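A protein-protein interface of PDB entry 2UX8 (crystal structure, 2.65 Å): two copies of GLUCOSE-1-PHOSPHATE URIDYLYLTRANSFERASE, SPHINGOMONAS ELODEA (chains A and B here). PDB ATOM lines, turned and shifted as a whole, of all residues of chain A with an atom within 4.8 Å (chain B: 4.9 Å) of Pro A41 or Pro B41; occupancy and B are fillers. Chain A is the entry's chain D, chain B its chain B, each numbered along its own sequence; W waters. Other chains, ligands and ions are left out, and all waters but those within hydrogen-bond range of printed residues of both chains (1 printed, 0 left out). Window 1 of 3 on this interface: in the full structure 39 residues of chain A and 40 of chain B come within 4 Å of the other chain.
Ala A31 touches Arg B45, and with the chains exchanged Arg A45 touches Ala B31. Ala A31 touches Pro B46, but with the chains exchanged Pro A46 does not touch Ala B31 (4.02 Å). Leu A40 touches Pro B41, and with the chains exchanged Pro A41 touches Leu B40. Pro B41 touches its own counterpart, Pro A41. Positions printed for both chains: 31, 39, 40, 41, 42, 43, 44, 45, 46, 270 and 274. Of the 9 pairs that touch across the chains among the printed residues, 7 have their exchanged pair printed and touching as well.
Pro A41 touches three residues of chain B. Of chain A, only Leu A40 (3.7 Å) and Pro A41 (3.8 Å) come within 4 Å of Pro B41. Of the printed residues of chain A, Leu B40 touches Pro A41 (3.7 Å). Of the printed residues of chain A, Arg B45 touches Ala A31 (3.9 Å). Of the printed residues of chain B, Leu A40 touches Pro B41 (3.7 Å). The nearest residue of chain B that does not touch Pro A41 is Phe B270 (4.2 Å). The nearest printed residue of chain A that does not touch Arg B45 is Leu A40 (7.8 Å).
Of the 11 printed residues of chain B, 6 touch a printed residue of chain A. Hydrophobic or aromatic side chains of chain B that line the printed part of chain A: Ala B31, Leu B40, Pro B41 and Pro B46. Of the 11 printed residues of chain A, 5 touch a printed residue of chain B. Printed residues of chain A that touch a printed residue of chain B: Ala A31, Leu A40, Pro A41, Asp A44 and Arg A45. Hydrophobic or aromatic side chains of chain A that line the printed part of chain B: Ala A31, Leu A40 and Pro A41. Along chain A the printed residues that touch a printed residue of chain B span positions 31 to 45.
ND2 of Asn B274 lies within hydrogen-bond range of O of Pro B41 (3.5 Å). ND2 of Asn A274 is in hydrogen-bond range of O of Pro A41, 3.3 Å away.
Among the printed residues, merely in contact across the chains: Pro A41 with Leu B40 (3.7 Å), Leu A40 with Pro B41 (3.7 Å), Pro A41 with Pro B41 (3.8 Å), Pro A41 with Ala B31 (3.9 Å), Ala A31 with Arg B45 (3.9 Å), Ala A31 with Pro B46 (3.96 Å) and Arg A45 with Ala B31 (3.99 Å).
Water W1 lies within hydrogen-bond range of the backbone carbonyl oxygen of Met B39 (2.8 Å) and the backbone carbonyl oxygen of Ala A31 (3.0 Å).
The backbone NH of Ala B31 sits at hydrogen-bond distance from the backbone carbonyl oxygen of Asp A44, 2.5 Å away. O of Asp B44 lies within hydrogen-bond range of N of Ala A31 (2.8 Å).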
ATOM      1  N   ALA A  31      14.903  19.203 -18.468  1.00  0.00           N
ATOM      2  CA  ALA A  31      14.381  18.714 -17.197  1.00  0.00           C
ATOM      3  C   ALA A  31      15.110  17.486 -16.675  1.00  0.00           C
ATOM      4  O   ALA A  31      15.297  17.324 -15.471  1.00  0.00           O
ATOM      5  CB  ALA A  31      12.897  18.400 -17.334  1.00  0.00           C
ATOM      6  N   MET A  39      11.834   9.996 -12.111  1.00  0.00           N
ATOM      7  CA  MET A  39      11.427  10.760 -10.948  1.00  0.00           C
ATOM      8  C   MET A  39      10.466  11.860 -11.326  1.00  0.00           C
ATOM      9  O   MET A  39       9.985  12.595 -10.447  1.00  0.00           O
ATOM     10  CB  MET A  39      12.639  11.362 -10.219  1.00  0.00           C
ATOM     11  CG  MET A  39      13.438  10.348  -9.411  1.00  0.00           C
ATOM     12  SD  MET A  39      12.459   9.452  -8.168  1.00  0.00           S
ATOM     13  CE  MET A  39      11.982  10.760  -7.059  1.00  0.00           C
ATOM     14  N   LEU A  40      10.179  11.981 -12.622  1.00  0.00           N
ATOM     15  CA  LEU A  40       9.247  13.019 -13.055  1.00  0.00           C
ATOM     16  C   LEU A  40       7.931  12.647 -12.382  1.00  0.00           C
ATOM     17  O   LEU A  40       7.567  11.446 -12.317  1.00  0.00           O
ATOM     18  CB  LEU A  40       9.053  13.046 -14.593  1.00  0.00           C
ATOM     19  CG  LEU A  40      10.292  13.545 -15.319  1.00  0.00           C
ATOM     20  CD1 LEU A  40       9.960  13.614 -16.779  1.00  0.00           C
ATOM     21  CD2 LEU A  40      10.723  14.896 -14.780  1.00  0.00           C
ATOM     22  N   PRO A  41       7.244  13.682 -11.823  1.00  0.00           N
ATOM     23  CA  PRO A  41       5.957  13.471 -11.158  1.00  0.00           C
ATOM     24  C   PRO A  41       4.632  13.666 -11.986  1.00  0.00           C
ATOM     25  O   PRO A  41       4.445  14.460 -12.866  1.00  0.00           O
ATOM     26  CB  PRO A  41       6.028  14.459 -10.008  1.00  0.00           C
ATOM     27  CG  PRO A  41       6.488  15.884 -10.952  1.00  0.00           C
ATOM     28  CD  PRO A  41       7.701  15.109 -11.694  1.00  0.00           C
ATOM     29  N   VAL A  42       3.702  12.804 -11.736  1.00  0.00           N
ATOM     30  CA  VAL A  42       2.406  13.035 -12.307  1.00  0.00           C
ATOM     31  C   VAL A  42       1.559  13.331 -11.085  1.00  0.00           C
ATOM     32  O   VAL A  42       1.202  12.491 -10.343  1.00  0.00           O
ATOM     33  CB  VAL A  42       1.940  11.901 -13.219  1.00  0.00           C
ATOM     34  CG1 VAL A  42       2.892  10.641 -13.179  1.00  0.00           C
ATOM     35  CG2 VAL A  42       0.425  11.596 -12.895  1.00  0.00           C
ATOM     36  N   VAL A  43       1.545  14.639 -10.894  1.00  0.00           N
ATOM     37  CA  VAL A  43       0.892  15.507  -9.927  1.00  0.00           C
ATOM     38  C   VAL A  43       1.630  15.427  -8.604  1.00  0.00           C
ATOM     39  O   VAL A  43       2.001  16.378  -7.931  1.00  0.00           O
ATOM     40  CB  VAL A  43      -0.612  15.011  -9.560  1.00  0.00           C
ATOM     41  CG1 VAL A  43      -1.205  15.905  -8.371  1.00  0.00           C
ATOM     42  CG2 VAL A  43      -1.567  14.866 -10.814  1.00  0.00           C
ATOM     43  N   ASP A  44       1.691  14.192  -8.141  1.00  0.00           N
ATOM     44  CA  ASP A  44       2.303  13.910  -6.790  1.00  0.00           C
ATOM     45  C   ASP A  44       3.433  12.973  -6.405  1.00  0.00           C
ATOM     46  O   ASP A  44       4.077  12.997  -5.338  1.00  0.00           O
ATOM     47  CB  ASP A  44       1.242  13.444  -5.810  1.00  0.00           C
ATOM     48  CG  ASP A  44       0.501  14.550  -5.186  1.00  0.00           C
ATOM     49  OD1 ASP A  44       1.031  15.701  -5.207  1.00  0.00           O
ATOM     50  OD2 ASP A  44      -0.593  14.198  -4.671  1.00  0.00           O
ATOM     51  N   ARG A  45       3.481  12.026  -7.275  1.00  0.00           N
ATOM     52  CA  ARG A  45       4.299  10.924  -7.152  1.00  0.00           C
ATOM     53  C   ARG A  45       5.065  10.733  -8.392  1.00  0.00           C
ATOM     54  O   ARG A  45       4.604  11.000  -9.498  1.00  0.00           O
ATOM     55  CB  ARG A  45       3.386   9.733  -6.865  1.00  0.00           C
ATOM     56  CG  ARG A  45       2.208  10.056  -5.918  1.00  0.00           C
ATOM     57  CD  ARG A  45       1.062   9.054  -6.086  1.00  0.00           C
ATOM     58  NE  ARG A  45       1.443   7.681  -5.765  1.00  0.00           N
ATOM     59  CZ  ARG A  45       1.565   7.214  -4.532  1.00  0.00           C
ATOM     60  NH1 ARG A  45       1.336   8.008  -3.507  1.00  0.00           N
ATOM     61  NH2 ARG A  45       1.916   5.959  -4.316  1.00  0.00           N
ATOM     62  N   PRO A  46       6.295  10.295  -8.202  1.00  0.00           N
ATOM     63  CA  PRO A  46       7.201  10.035  -9.306  1.00  0.00           C
ATOM     64  C   PRO A  46       6.736   8.791 -10.065  1.00  0.00           C
ATOM     65  O   PRO A  46       6.154   7.874  -9.480  1.00  0.00           O
ATOM     66  CB  PRO A  46       8.531   9.841  -8.598  1.00  0.00           C
ATOM     67  CG  PRO A  46       8.112   9.218  -7.278  1.00  0.00           C
ATOM     68  CD  PRO A  46       6.935  10.058  -6.894  1.00  0.00           C
ATOM     69  N   PHE A 270       3.007  12.981 -20.992  1.00  0.00           N
ATOM     70  CA  PHE A 270       3.277  13.364 -19.616  1.00  0.00           C
ATOM     71  C   PHE A 270       2.244  14.389 -19.141  1.00  0.00           C
ATOM     72  O   PHE A 270       1.710  14.289 -18.036  1.00  0.00           O
ATOM     73  CB  PHE A 270       4.692  13.947 -19.513  1.00  0.00           C
ATOM     74  CG  PHE A 270       5.024  14.515 -18.156  1.00  0.00           C
ATOM     75  CD1 PHE A 270       5.184  13.682 -17.053  1.00  0.00           C
ATOM     76  CD2 PHE A 270       5.158  15.890 -17.982  1.00  0.00           C
ATOM     77  CE1 PHE A 270       5.470  14.207 -15.796  1.00  0.00           C
ATOM     78  CE2 PHE A 270       5.444  16.429 -16.727  1.00  0.00           C
ATOM     79  CZ  PHE A 270       5.599  15.586 -15.631  1.00  0.00           C
ATOM     80  N   ASN A 274      -0.866  13.960 -16.323  1.00  0.00           N
ATOM     81  CA  ASN A 274      -0.992  14.882 -15.204  1.00  0.00           C
ATOM     82  C   ASN A 274      -2.391  15.465 -15.092  1.00  0.00           C
ATOM     83  O   ASN A 274      -2.922  15.623 -13.994  1.00  0.00           O
ATOM     84  CB  ASN A 274       0.023  16.015 -15.348  1.00  0.00           C
ATOM     85  CG  ASN A 274       1.279  15.754 -14.573  1.00  0.00           C
ATOM     86  OD1 ASN A 274       1.327  15.975 -13.376  1.00  0.00           O
ATOM     87  ND2 ASN A 274       2.295  15.254 -15.246  1.00  0.00           N
ATOM     88  N   ALA B  31       6.228  13.308  -4.015  1.00  0.00           N
ATOM     89  CA  ALA B  31       7.090  13.666  -5.132  1.00  0.00           C
ATOM     90  C   ALA B  31       8.365  14.354  -4.682  1.00  0.00           C
ATOM     91  O   ALA B  31       9.436  14.140  -5.248  1.00  0.00           O
ATOM     92  CB  ALA B  31       6.341  14.558  -6.127  1.00  0.00           C
ATOM     93  N   MET B  39      12.985  21.503  -8.513  1.00  0.00           N
ATOM     94  CA  MET B  39      13.333  20.750  -9.701  1.00  0.00           C
ATOM     95  C   MET B  39      12.122  20.170 -10.425  1.00  0.00           C
ATOM     96  O   MET B  39      12.277  19.538 -11.464  1.00  0.00           O
ATOM     97  CB  MET B  39      14.316  19.624  -9.361  1.00  0.00           C
ATOM     98  CG  MET B  39      15.739  20.075  -9.033  1.00  0.00           C
ATOM     99  SD  MET B  39      16.564  20.906 -10.402  1.00  0.00           S
ATOM    100  CE  MET B  39      16.832  19.557 -11.535  1.00  0.00           C
ATOM    101  N   LEU B  40      10.924  20.368  -9.882  1.00  0.00           N
ATOM    102  CA  LEU B  40       9.738  19.865 -10.556  1.00  0.00           C
ATOM    103  C   LEU B  40       9.623  20.597 -11.886  1.00  0.00           C
ATOM    104  O   LEU B  40       9.787  21.818 -11.966  1.00  0.00           O
ATOM    105  CB  LEU B  40       8.466  20.072  -9.723  1.00  0.00           C
ATOM    106  CG  LEU B  40       8.388  19.227  -8.446  1.00  0.00           C
ATOM    107  CD1 LEU B  40       6.995  19.333  -7.834  1.00  0.00           C
ATOM    108  CD2 LEU B  40       8.722  17.775  -8.756  1.00  0.00           C
ATOM    109  N   PRO B  41       9.343  19.847 -12.956  1.00  0.00           N
ATOM    110  CA  PRO B  41       9.212  20.397 -14.297  1.00  0.00           C
ATOM    111  C   PRO B  41       7.856  20.964 -14.673  1.00  0.00           C
ATOM    112  O   PRO B  41       6.825  20.414 -14.297  1.00  0.00           O
ATOM    113  CB  PRO B  41       9.528  19.193 -15.172  1.00  0.00           C
ATOM    114  CG  PRO B  41       8.818  18.103 -14.435  1.00  0.00           C
ATOM    115  CD  PRO B  41       9.223  18.375 -12.992  1.00  0.00           C
ATOM    116  N   VAL B  42       7.886  22.076 -15.409  1.00  0.00           N
ATOM    117  CA  VAL B  42       6.688  22.659 -16.001  1.00  0.00           C
ATOM    118  C   VAL B  42       6.926  22.291 -17.478  1.00  0.00           C
ATOM    119  O   VAL B  42       7.513  23.050 -18.247  1.00  0.00           O
ATOM    120  CB  VAL B  42       6.630  24.173 -15.918  1.00  0.00           C
ATOM    121  CG1 VAL B  42       5.448  24.646 -16.700  1.00  0.00           C
ATOM    122  CG2 VAL B  42       6.514  24.630 -14.493  1.00  0.00           C
ATOM    123  N   VAL B  43       6.504  21.087 -17.841  1.00  0.00           N
ATOM    124  CA  VAL B  43       6.654  20.530 -19.183  1.00  0.00           C
ATOM    125  C   VAL B  43       8.031  19.900 -19.379  1.00  0.00           C
ATOM    126  O   VAL B  43       8.165  18.686 -19.503  1.00  0.00           O
ATOM    127  CB  VAL B  43       6.500  21.587 -20.286  1.00  0.00           C
ATOM    128  CG1 VAL B  43       6.630  20.931 -21.646  1.00  0.00           C
ATOM    129  CG2 VAL B  43       5.187  22.322 -20.156  1.00  0.00           C
ATOM    130  N   ASP B  44       9.070  20.721 -19.457  1.00  0.00           N
ATOM    131  CA  ASP B  44      10.384  20.127 -19.671  1.00  0.00           C
ATOM    132  C   ASP B  44      11.572  20.885 -19.155  1.00  0.00           C
ATOM    133  O   ASP B  44      12.714  20.634 -19.552  1.00  0.00           O
ATOM    134  CB  ASP B  44      10.589  19.737 -21.140  1.00  0.00           C
ATOM    135  CG  ASP B  44      10.387  20.882 -22.067  1.00  0.00           C
ATOM    136  OD1 ASP B  44       9.871  21.901 -21.593  1.00  0.00           O
ATOM    137  OD2 ASP B  44      10.727  20.776 -23.261  1.00  0.00           O
ATOM    138  N   ARG B  45      11.284  21.832 -18.279  1.00  0.00           N
ATOM    139  CA  ARG B  45      12.332  22.549 -17.594  1.00  0.00           C
ATOM    140  C   ARG B  45      11.879  22.739 -16.156  1.00  0.00           C
ATOM    141  O   ARG B  45      10.696  22.957 -15.886  1.00  0.00           O
ATOM    142  CB  ARG B  45      12.665  23.889 -18.249  1.00  0.00           C
ATOM    143  CG  ARG B  45      11.651  24.420 -19.208  1.00  0.00           C
ATOM    144  CD  ARG B  45      12.196  25.661 -19.893  1.00  0.00           C
ATOM    145  NE  ARG B  45      13.179  25.315 -20.916  1.00  0.00           N
ATOM    146  CZ  ARG B  45      14.340  25.940 -21.101  1.00  0.00           C
ATOM    147  NH1 ARG B  45      14.687  26.957 -20.330  1.00  0.00           N
ATOM    148  NH2 ARG B  45      15.159  25.548 -22.065  1.00  0.00           N
ATOM    149  N   PRO B  46      12.814  22.602 -15.201  1.00  0.00           N
ATOM    150  CA  PRO B  46      12.506  22.764 -13.777  1.00  0.00           C
ATOM    151  C   PRO B  46      12.224  24.216 -13.394  1.00  0.00           C
ATOM    152  O   PRO B  46      12.739  25.147 -14.016  1.00  0.00           O
ATOM    153  CB  PRO B  46      13.761  22.240 -13.094  1.00  0.00           C
ATOM    154  CG  PRO B  46      14.839  22.627 -14.065  1.00  0.00           C
ATOM    155  CD  PRO B  46      14.229  22.235 -15.391  1.00  0.00           C
ATOM    156  N   PHE B 270       0.396  24.043 -10.138  1.00  0.00           N
ATOM    157  CA  PHE B 270       1.430  23.316 -10.869  1.00  0.00           C
ATOM    158  C   PHE B 270       0.860  22.696 -12.143  1.00  0.00           C
ATOM    159  O   PHE B 270       1.463  22.782 -13.211  1.00  0.00           O
ATOM    160  CB  PHE B 270       2.012  22.219  -9.970  1.00  0.00           C
ATOM    161  CG  PHE B 270       2.992  21.310 -10.663  1.00  0.00           C
ATOM    162  CD1 PHE B 270       4.257  21.767 -11.031  1.00  0.00           C
ATOM    163  CD2 PHE B 270       2.654  19.987 -10.931  1.00  0.00           C
ATOM    164  CE1 PHE B 270       5.171  20.916 -11.656  1.00  0.00           C
ATOM    165  CE2 PHE B 270       3.560  19.131 -11.554  1.00  0.00           C
ATOM    166  CZ  PHE B 270       4.822  19.599 -11.917  1.00  0.00           C
ATOM    167  N   ASN B 274       1.477  23.724 -16.185  1.00  0.00           N
ATOM    168  CA  ASN B 274       1.923  22.763 -17.170  1.00  0.00           C
ATOM    169  C   ASN B 274       1.018  22.760 -18.385  1.00  0.00           C
ATOM    170  O   ASN B 274       1.473  22.579 -19.517  1.00  0.00           O
ATOM    171  CB  ASN B 274       1.967  21.367 -16.549  1.00  0.00           C
ATOM    172  CG  ASN B 274       3.326  21.028 -15.970  1.00  0.00           C
ATOM    173  OD1 ASN B 274       4.230  20.607 -16.686  1.00  0.00           O
ATOM    174  ND2 ASN B 274       3.478  21.221 -14.669  1.00  0.00           N
HETATM  175  O   HOH W   1      13.364  19.155 -14.033  1.00  0.00           O
